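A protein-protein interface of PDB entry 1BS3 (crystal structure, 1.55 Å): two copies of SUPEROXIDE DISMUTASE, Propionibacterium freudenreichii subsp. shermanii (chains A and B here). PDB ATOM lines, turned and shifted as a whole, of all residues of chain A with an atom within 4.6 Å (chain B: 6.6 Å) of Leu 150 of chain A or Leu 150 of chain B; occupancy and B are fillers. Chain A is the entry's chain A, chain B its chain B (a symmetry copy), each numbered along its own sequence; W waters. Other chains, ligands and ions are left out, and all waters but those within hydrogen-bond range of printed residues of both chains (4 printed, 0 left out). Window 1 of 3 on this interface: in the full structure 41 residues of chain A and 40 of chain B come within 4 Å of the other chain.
The backbone NH of Asn 149 of chain B sits at hydrogen-bond distance from the backbone carbonyl oxygen of Gln 147 of chain A (3.0 Å). N of Leu 150 of chain B is in hydrogen-bond range of O of Gln 147 of chain A (3.0 Å). The side-chain amide oxygen (OD1) of Asn 148 of chain A is in hydrogen-bond range of the backbone NH (N) of Asn 149 of chain B (2.9 Å). The backbone NH (N) of Asn 149 of chain A sits at hydrogen-bond distance from the backbone carbonyl oxygen (O) of Gln 147 of chain B (2.9 Å). The backbone NH (N) of Asn 149 of chain A sits at hydrogen-bond distance from the side-chain amide oxygen (OD1) of Asn 148 of chain B, 2.9 Å away. The backbone NH (N) of Leu 150 of chain A sits at hydrogen-bond distance from the backbone carbonyl oxygen (O) of Gln 147 of chain B (3.0 Å).
Hydrophobic or aromatic side chains of chain A within 4 Å of the printed part of chain B: Ala 66, Ala 70, Leu 150, Pro 151 and Ala 152. Among the printed residues, no Asp or Glu carboxylate lies within 4 Å of a Lys or Arg side-chain nitrogen of the other chain.
Water W1 lies within hydrogen-bond range of OD1 of Asn 149 of chain A (2.7 Å), NE2 of Gln 147 of chain B (2.8 Å) and OD1 of Asn 148 of chain B (2.9 Å). Water W3 lies within hydrogen-bond range of OD1 of Asn 74 of chain B (2.8 Å), N of Ala 152 of chain A (2.8 Å) and O of His 146 of chain B (2.9 Å). Water W2 lies within hydrogen-bond range of the side-chain amide oxygen (OD1) of Asn 148 of chain A (2.8 Å), the side-chain amide oxygen (OD1) of Asn 149 of chain B (2.9 Å) and the side-chain amide nitrogen (NE2) of Gln 147 of chain A (3.0 Å). Water W4 lies within hydrogen-bond range of O of Pro 151 of chain B (3.0 Å), O of Pro 151 of chain A (3.2 Å), N of Gly 153 of chain B (3.2 Å) and N of Ser 154 of chain B (3.5 Å).
Ala 66 of chain A touches Asn 149 of chain B, and with the chains exchanged Asn 149 of chain A touches Ala 66 of chain B. Ala 66 of chain A touches Leu 150 of chain B, and with the chains exchanged Leu 150 of chain A touches Ala 66 of chain B. Gln 147 of chain A touches Asn 148 of chain B, and with the chains exchanged Asn 148 of chain A touches Gln 147 of chain B. Gln 147 of chain A touches Asn 149 of chain B, and with the chains exchanged Asn 149 of chain A touches Gln 147 of chain B.
ND2 of Asn 74 of chain B sits close to O of Ala 70 of chain B, 3.3 Å away. ND2 of Asn 149 of chain B lies within hydrogen-bond range of O of Gln 142 of chain B (2.7 Å). OG of Ser 154 of chain B is in hydrogen-bond range of O of Pro 151 of chain B, at 2.6 Å.
Of the printed residues of chain B, Ala 66 of chain A touches Asn 149, Leu 150 and Pro 151. Leu 150 of chain A touches just these residues of chain B: Ala 66 (3.96 Å), Gln 147 (3.0 Å), Leu 150 (3.5 Å) and Ala 152 (3.4 Å). Of the printed residues of chain A, Asn 149 of chain B touches Ala 66 (3.3 Å), Gln 147 (3.0 Å) and Asn 148 (2.9 Å). Of chain A, only Ala 66, Gln 147, Leu 150 and Ala 152 come within 4 Å of Leu 150 of chain B. Of the printed residues of chain A, Pro 151 of chain B touches Ala 66 and Ala 70. Printed residues of chain A within 4 Å of Ser 154 of chain B: Ala 152. The nearest printed residue of chain B that does not touch Asn 149 of chain A is Phe 67 of chain B (5.1 Å).
Among the printed residues, merely in contact across the chains: Ala 66 of chain A with Asn 149 of chain B (3.3 Å), Ala 66 of chain A with Leu 150 of chain B (3.9 Å), Ala 66 of chain A with Pro 151 of chain B (3.95 Å), Ala 70 of chain A with Pro 151 of chain B (3.8 Å), Gln 147 of chain A with Asn 148 of chain B (3.8 Å), Asn 148 of chain A with Gln 147 of chain B (3.7 Å), Asn 148 of chain A with Asn 148 of chain B (3.3 Å), Asn 149 of chain A with Ala 66 of chain B (3.3 Å), Leu 150 of chain A with Ala 66 of chain B (3.96 Å), Leu 150 of chain A with Leu 150 of chain B (3.5 Å), Leu 150 of chain A with Ala 152 of chain B (3.4 Å), Pro 151 of chain A with Ala 66 of chain B (3.9 Å), Pro 151 of chain A with Ala 70 of chain B (3.8 Å), Ala 152 of chain A with Leu 150 of chain B (3.5 Å) and Ala 152 of chain A with Ser 154 of chain B (3.9 Å).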
ATOM      1  N   ALA A  66       7.132  14.846 -15.197  1.00  0.00           N
ATOM      2  CA  ALA A  66       6.595  14.667 -16.546  1.00  0.00           C
ATOM      3  C   ALA A  66       7.444  13.725 -17.399  1.00  0.00           C
ATOM      4  O   ALA A  66       6.915  12.819 -18.043  1.00  0.00           O
ATOM      5  CB  ALA A  66       6.449  16.011 -17.239  1.00  0.00           C
ATOM      6  N   ALA A  70       6.076  10.046 -17.978  1.00  0.00           N
ATOM      7  CA  ALA A  70       5.754   9.832 -19.384  1.00  0.00           C
ATOM      8  C   ALA A  70       6.541   8.624 -19.894  1.00  0.00           C
ATOM      9  O   ALA A  70       6.022   7.818 -20.656  1.00  0.00           O
ATOM     10  CB  ALA A  70       6.087  11.057 -20.203  1.00  0.00           C
ATOM     11  N   LEU A 141       0.227  10.809 -33.330  1.00  0.00           N
ATOM     12  CA  LEU A 141       0.959  11.896 -32.709  1.00  0.00           C
ATOM     13  C   LEU A 141       2.429  11.525 -32.716  1.00  0.00           C
ATOM     14  O   LEU A 141       2.785  10.348 -32.721  1.00  0.00           O
ATOM     15  CB  LEU A 141       0.502  12.115 -31.265  1.00  0.00           C
ATOM     16  CG  LEU A 141      -0.921  12.628 -31.055  1.00  0.00           C
ATOM     17  CD1 LEU A 141      -1.179  12.771 -29.558  1.00  0.00           C
ATOM     18  CD2 LEU A 141      -1.115  13.965 -31.766  1.00  0.00           C
ATOM     19  N   PHE A 143       5.499  12.136 -30.454  1.00  0.00           N
ATOM     20  CA  PHE A 143       6.007  12.620 -29.174  1.00  0.00           C
ATOM     21  C   PHE A 143       7.485  12.964 -29.309  1.00  0.00           C
ATOM     22  O   PHE A 143       8.219  12.293 -30.043  1.00  0.00           O
ATOM     23  CB  PHE A 143       5.914  11.538 -28.083  1.00  0.00           C
ATOM     24  CG  PHE A 143       4.515  11.075 -27.752  1.00  0.00           C
ATOM     25  CD1 PHE A 143       3.393  11.609 -28.384  1.00  0.00           C
ATOM     26  CD2 PHE A 143       4.332  10.075 -26.800  1.00  0.00           C
ATOM     27  CE1 PHE A 143       2.114  11.156 -28.069  1.00  0.00           C
ATOM     28  CE2 PHE A 143       3.055   9.615 -26.475  1.00  0.00           C
ATOM     29  CZ  PHE A 143       1.944  10.155 -27.115  1.00  0.00           C
ATOM     30  N   GLN A 147       7.523  13.186 -23.064  1.00  0.00           N
ATOM     31  CA  GLN A 147       6.458  14.055 -22.605  1.00  0.00           C
ATOM     32  C   GLN A 147       6.096  15.301 -23.412  1.00  0.00           C
ATOM     33  O   GLN A 147       5.344  16.150 -22.930  1.00  0.00           O
ATOM     34  CB  GLN A 147       6.804  14.459 -21.165  1.00  0.00           C
ATOM     35  CG  GLN A 147       7.923  15.524 -21.021  1.00  0.00           C
ATOM     36  CD  GLN A 147       9.362  15.059 -21.328  1.00  0.00           C
ATOM     37  OE1 GLN A 147       9.593  13.963 -21.839  1.00  0.00           O
ATOM     38  NE2 GLN A 147      10.329  15.907 -21.005  1.00  0.00           N
ATOM     39  N   ASN A 148       6.605  15.416 -24.632  1.00  0.00           N
ATOM     40  CA  ASN A 148       6.306  16.594 -25.432  1.00  0.00           C
ATOM     41  C   ASN A 148       5.555  16.316 -26.722  1.00  0.00           C
ATOM     42  O   ASN A 148       5.587  15.207 -27.257  1.00  0.00           O
ATOM     43  CB  ASN A 148       7.595  17.351 -25.755  1.00  0.00           C
ATOM     44  CG  ASN A 148       8.350  17.772 -24.519  1.00  0.00           C
ATOM     45  OD1 ASN A 148       7.763  18.205 -23.534  1.00  0.00           O
ATOM     46  ND2 ASN A 148       9.665  17.645 -24.565  1.00  0.00           N
ATOM     47  N   ASN A 149       4.878  17.354 -27.202  1.00  0.00           N
ATOM     48  CA  ASN A 149       4.121  17.325 -28.445  1.00  0.00           C
ATOM     49  C   ASN A 149       2.853  16.463 -28.431  1.00  0.00           C
ATOM     50  O   ASN A 149       2.581  15.724 -29.380  1.00  0.00           O
ATOM     51  CB  ASN A 149       5.043  16.934 -29.611  1.00  0.00           C
ATOM     52  CG  ASN A 149       4.668  17.625 -30.908  1.00  0.00           C
ATOM     53  OD1 ASN A 149       4.343  18.815 -30.917  1.00  0.00           O
ATOM     54  ND2 ASN A 149       4.718  16.889 -32.011  1.00  0.00           N
ATOM     55  N   LEU A 150       2.052  16.609 -27.376  1.00  0.00           N
ATOM     56  CA  LEU A 150       0.805  15.853 -27.256  1.00  0.00           C
ATOM     57  C   LEU A 150      -0.221  16.603 -26.411  1.00  0.00           C
ATOM     58  O   LEU A 150       0.133  17.300 -25.462  1.00  0.00           O
ATOM     59  CB  LEU A 150       1.051  14.477 -26.627  1.00  0.00           C
ATOM     60  CG  LEU A 150       1.443  14.445 -25.143  1.00  0.00           C
ATOM     61  CD1 LEU A 150       0.928  13.173 -24.488  1.00  0.00           C
ATOM     62  CD2 LEU A 150       2.950  14.570 -24.987  1.00  0.00           C
ATOM     63  N   PRO A 151      -1.511  16.481 -26.771  1.00  0.00           N
ATOM     64  CA  PRO A 151      -2.590  17.142 -26.027  1.00  0.00           C
ATOM     65  C   PRO A 151      -2.909  16.358 -24.761  1.00  0.00           C
ATOM     66  O   PRO A 151      -2.759  15.137 -24.726  1.00  0.00           O
ATOM     67  CB  PRO A 151      -3.770  17.057 -27.004  1.00  0.00           C
ATOM     68  CG  PRO A 151      -3.129  16.930 -28.342  1.00  0.00           C
ATOM     69  CD  PRO A 151      -2.008  15.969 -28.050  1.00  0.00           C
ATOM     70  N   ALA A 152      -3.332  17.058 -23.713  1.00  0.00           N
ATOM     71  CA  ALA A 152      -3.708  16.403 -22.467  1.00  0.00           C
ATOM     72  C   ALA A 152      -4.948  15.573 -22.781  1.00  0.00           C
ATOM     73  O   ALA A 152      -5.729  15.931 -23.668  1.00  0.00           O
ATOM     74  CB  ALA A 152      -4.032  17.445 -21.396  1.00  0.00           C
ATOM     75  N   ALA B  66      -0.783  18.782 -32.560  1.00  0.00           N
ATOM     76  CA  ALA B  66      -0.565  18.762 -31.116  1.00  0.00           C
ATOM     77  C   ALA B  66      -0.724  20.132 -30.459  1.00  0.00           C
ATOM     78  O   ALA B  66      -1.385  20.253 -29.428  1.00  0.00           O
ATOM     79  CB  ALA B  66       0.803  18.166 -30.791  1.00  0.00           C
ATOM     80  N   PHE B  67      -0.136  21.159 -31.066  1.00  0.00           N
ATOM     81  CA  PHE B  67      -0.211  22.515 -30.534  1.00  0.00           C
ATOM     82  C   PHE B  67      -1.644  23.040 -30.517  1.00  0.00           C
ATOM     83  O   PHE B  67      -2.128  23.508 -29.488  1.00  0.00           O
ATOM     84  CB  PHE B  67       0.680  23.460 -31.348  1.00  0.00           C
ATOM     85  CG  PHE B  67       0.569  24.905 -30.938  1.00  0.00           C
ATOM     86  CD1 PHE B  67       1.146  25.352 -29.753  1.00  0.00           C
ATOM     87  CD2 PHE B  67      -0.121  25.815 -31.733  1.00  0.00           C
ATOM     88  CE1 PHE B  67       1.036  26.683 -29.365  1.00  0.00           C
ATOM     89  CE2 PHE B  67      -0.237  27.148 -31.355  1.00  0.00           C
ATOM     90  CZ  PHE B  67       0.342  27.584 -30.168  1.00  0.00           C
ATOM     91  N   ALA B  70      -4.147  20.720 -28.465  1.00  0.00           N
ATOM     92  CA  ALA B  70      -3.873  20.927 -27.044  1.00  0.00           C
ATOM     93  C   ALA B  70      -4.414  22.288 -26.610  1.00  0.00           C
ATOM     94  O   ALA B  70      -4.925  22.427 -25.500  1.00  0.00           O
ATOM     95  CB  ALA B  70      -2.388  20.839 -26.757  1.00  0.00           C
ATOM     96  N   ASN B  74      -7.142  22.457 -23.669  1.00  0.00           N
ATOM     97  CA  ASN B  74      -6.822  23.267 -22.499  1.00  0.00           C
ATOM     98  C   ASN B  74      -7.817  24.389 -22.232  1.00  0.00           C
ATOM     99  O   ASN B  74      -8.240  24.588 -21.093  1.00  0.00           O
ATOM    100  CB  ASN B  74      -5.411  23.848 -22.620  1.00  0.00           C
ATOM    101  CG  ASN B  74      -4.332  22.782 -22.617  1.00  0.00           C
ATOM    102  OD1 ASN B  74      -4.594  21.603 -22.355  1.00  0.00           O
ATOM    103  ND2 ASN B  74      -3.099  23.196 -22.907  1.00  0.00           N
ATOM    104  N   LEU B 141       0.905  19.355 -12.809  1.00  0.00           N
ATOM    105  CA  LEU B 141       1.847  19.348 -13.918  1.00  0.00           C
ATOM    106  C   LEU B 141       2.010  20.788 -14.362  1.00  0.00           C
ATOM    107  O   LEU B 141       1.151  21.632 -14.085  1.00  0.00           O
ATOM    108  CB  LEU B 141       1.322  18.522 -15.092  1.00  0.00           C
ATOM    109  CG  LEU B 141       1.237  17.004 -14.925  1.00  0.00           C
ATOM    110  CD1 LEU B 141       0.639  16.409 -16.189  1.00  0.00           C
ATOM    111  CD2 LEU B 141       2.624  16.416 -14.653  1.00  0.00           C
ATOM    112  N   GLN B 142       3.119  21.063 -15.037  1.00  0.00           N
ATOM    113  CA  GLN B 142       3.401  22.396 -15.549  1.00  0.00           C
ATOM    114  C   GLN B 142       3.592  22.249 -17.054  1.00  0.00           C
ATOM    115  O   GLN B 142       4.638  21.776 -17.507  1.00  0.00           O
ATOM    116  CB  GLN B 142       4.674  22.946 -14.899  1.00  0.00           C
ATOM    117  CG  GLN B 142       5.013  24.381 -15.265  1.00  0.00           C
ATOM    118  CD  GLN B 142       6.383  24.791 -14.752  1.00  0.00           C
ATOM    119  OE1 GLN B 142       7.410  24.363 -15.284  1.00  0.00           O
ATOM    120  NE2 GLN B 142       6.408  25.619 -13.711  1.00  0.00           N
ATOM    121  N   PHE B 143       2.558  22.576 -17.828  1.00  0.00           N
ATOM    122  CA  PHE B 143       2.646  22.465 -19.285  1.00  0.00           C
ATOM    123  C   PHE B 143       3.464  23.618 -19.851  1.00  0.00           C
ATOM    124  O   PHE B 143       3.436  24.724 -19.316  1.00  0.00           O
ATOM    125  CB  PHE B 143       1.266  22.562 -19.959  1.00  0.00           C
ATOM    126  CG  PHE B 143       0.290  21.484 -19.578  1.00  0.00           C
ATOM    127  CD1 PHE B 143       0.656  20.403 -18.778  1.00  0.00           C
ATOM    128  CD2 PHE B 143      -1.024  21.564 -20.028  1.00  0.00           C
ATOM    129  CE1 PHE B 143      -0.276  19.422 -18.434  1.00  0.00           C
ATOM    130  CE2 PHE B 143      -1.962  20.593 -19.692  1.00  0.00           C
ATOM    131  CZ  PHE B 143      -1.588  19.518 -18.893  1.00  0.00           C
ATOM    132  N   TYR B 144       4.212  23.339 -20.915  1.00  0.00           N
ATOM    133  CA  TYR B 144       4.972  24.366 -21.625  1.00  0.00           C
ATOM    134  C   TYR B 144       4.111  24.565 -22.870  1.00  0.00           C
ATOM    135  O   TYR B 144       3.676  23.586 -23.489  1.00  0.00           O
ATOM    136  CB  TYR B 144       6.357  23.879 -22.048  1.00  0.00           C
ATOM    137  CG  TYR B 144       7.270  23.450 -20.927  1.00  0.00           C
ATOM    138  CD1 TYR B 144       7.037  23.833 -19.605  1.00  0.00           C
ATOM    139  CD2 TYR B 144       8.379  22.653 -21.195  1.00  0.00           C
ATOM    140  CE1 TYR B 144       7.892  23.423 -18.577  1.00  0.00           C
ATOM    141  CE2 TYR B 144       9.232  22.240 -20.187  1.00  0.00           C
ATOM    142  CZ  TYR B 144       8.991  22.623 -18.883  1.00  0.00           C
ATOM    143  OH  TYR B 144       9.857  22.207 -17.896  1.00  0.00           O
ATOM    144  N   HIS B 146       1.248  24.552 -24.936  1.00  0.00           N
ATOM    145  CA  HIS B 146      -0.032  23.867 -24.710  1.00  0.00           C
ATOM    146  C   HIS B 146       0.138  22.356 -24.659  1.00  0.00           C
ATOM    147  O   HIS B 146      -0.574  21.664 -23.928  1.00  0.00           O
ATOM    148  CB  HIS B 146      -1.011  24.122 -25.860  1.00  0.00           C
ATOM    149  CG  HIS B 146      -1.485  25.532 -25.963  1.00  0.00           C
ATOM    150  ND1 HIS B 146      -1.536  26.209 -27.160  1.00  0.00           N
ATOM    151  CD2 HIS B 146      -1.940  26.388 -25.022  1.00  0.00           C
ATOM    152  CE1 HIS B 146      -2.005  27.426 -26.950  1.00  0.00           C
ATOM    153  NE2 HIS B 146      -2.257  27.559 -25.662  1.00  0.00           N
ATOM    154  N   GLN B 147       1.140  21.882 -25.393  1.00  0.00           N
ATOM    155  CA  GLN B 147       1.375  20.462 -25.600  1.00  0.00           C
ATOM    156  C   GLN B 147       2.655  19.828 -25.076  1.00  0.00           C
ATOM    157  O   GLN B 147       2.973  18.702 -25.446  1.00  0.00           O
ATOM    158  CB  GLN B 147       1.274  20.202 -27.111  1.00  0.00           C
ATOM    159  CG  GLN B 147       2.495  20.658 -27.964  1.00  0.00           C
ATOM    160  CD  GLN B 147       2.752  22.182 -28.043  1.00  0.00           C
ATOM    161  OE1 GLN B 147       1.994  23.000 -27.517  1.00  0.00           O
ATOM    162  NE2 GLN B 147       3.835  22.554 -28.711  1.00  0.00           N
ATOM    163  N   ASN B 148       3.390  20.528 -24.222  1.00  0.00           N
ATOM    164  CA  ASN B 148       4.640  19.975 -23.716  1.00  0.00           C
ATOM    165  C   ASN B 148       4.700  19.801 -22.208  1.00  0.00           C
ATOM    166  O   ASN B 148       3.980  20.468 -21.466  1.00  0.00           O
ATOM    167  CB  ASN B 148       5.823  20.843 -24.161  1.00  0.00           C
ATOM    168  CG  ASN B 148       5.911  20.995 -25.674  1.00  0.00           C
ATOM    169  OD1 ASN B 148       5.611  20.071 -26.424  1.00  0.00           O
ATOM    170  ND2 ASN B 148       6.330  22.167 -26.122  1.00  0.00           N
ATOM    171  N   ASN B 149       5.565  18.881 -21.782  1.00  0.00           N
ATOM    172  CA  ASN B 149       5.814  18.578 -20.371  1.00  0.00           C
ATOM    173  C   ASN B 149       4.660  17.868 -19.646  1.00  0.00           C
ATOM    174  O   ASN B 149       4.322  18.206 -18.505  1.00  0.00           O
ATOM    175  CB  ASN B 149       6.233  19.860 -19.631  1.00  0.00           C
ATOM    176  CG  ASN B 149       7.153  19.592 -18.444  1.00  0.00           C
ATOM    177  OD1 ASN B 149       8.057  18.756 -18.522  1.00  0.00           O
ATOM    178  ND2 ASN B 149       6.908  20.276 -17.332  1.00  0.00           N
ATOM    179  N   LEU B 150       4.101  16.845 -20.292  1.00  0.00           N
ATOM    180  CA  LEU B 150       2.996  16.077 -19.712  1.00  0.00           C
ATOM    181  C   LEU B 150       2.960  14.635 -20.230  1.00  0.00           C
ATOM    182  O   LEU B 150       3.324  14.371 -21.378  1.00  0.00           O
ATOM    183  CB  LEU B 150       1.646  16.745 -20.027  1.00  0.00           C
ATOM    184  CG  LEU B 150       1.095  16.644 -21.459  1.00  0.00           C
ATOM    185  CD1 LEU B 150      -0.410  16.870 -21.458  1.00  0.00           C
ATOM    186  CD2 LEU B 150       1.786  17.628 -22.379  1.00  0.00           C
ATOM    187  N   PRO B 151       2.565  13.679 -19.367  1.00  0.00           N
ATOM    188  CA  PRO B 151       2.485  12.269 -19.779  1.00  0.00           C
ATOM    189  C   PRO B 151       1.185  12.014 -20.535  1.00  0.00           C
ATOM    190  O   PRO B 151       0.157  12.632 -20.239  1.00  0.00           O
ATOM    191  CB  PRO B 151       2.447  11.517 -18.438  1.00  0.00           C
ATOM    192  CG  PRO B 151       3.022  12.485 -17.450  1.00  0.00           C
ATOM    193  CD  PRO B 151       2.462  13.800 -17.907  1.00  0.00           C
ATOM    194  N   ALA B 152       1.226  11.111 -21.510  1.00  0.00           N
ATOM    195  CA  ALA B 152       0.025  10.756 -22.260  1.00  0.00           C
ATOM    196  C   ALA B 152      -0.939  10.102 -21.271  1.00  0.00           C
ATOM    197  O   ALA B 152      -0.511   9.443 -20.317  1.00  0.00           O
ATOM    198  CB  ALA B 152       0.360   9.781 -23.380  1.00  0.00           C
ATOM    199  N   GLY B 153      -2.234  10.318 -21.470  1.00  0.00           N
ATOM    200  CA  GLY B 153      -3.218   9.728 -20.578  1.00  0.00           C
ATOM    201  C   GLY B 153      -3.584  10.575 -19.370  1.00  0.00           C
ATOM    202  O   GLY B 153      -4.423  10.169 -18.565  1.00  0.00           O
ATOM    203  N   SER B 154      -2.948  11.737 -19.227  1.00  0.00           N
ATOM    204  CA  SER B 154      -3.243  12.640 -18.116  1.00  0.00           C
ATOM    205  C   SER B 154      -4.637  13.220 -18.316  1.00  0.00           C
ATOM    206  O   SER B 154      -4.954  13.714 -19.398  1.00  0.00           O
ATOM    207  CB  SER B 154      -2.233  13.789 -18.069  1.00  0.00           C
ATOM    208  OG  SER B 154      -0.910  13.306 -17.934  1.00  0.00           O
HETATM  209  O   HOH W   1       5.703  20.487 -29.284  1.00  0.00           O
HETATM  210  O   HOH W   2       9.281  18.728 -21.195  1.00  0.00           O
HETATM  211  O   HOH W   3      -2.797  19.801 -23.444  1.00  0.00           O
HETATM  212  O   HOH W   4      -2.087  13.415 -22.147  1.00  0.00           O
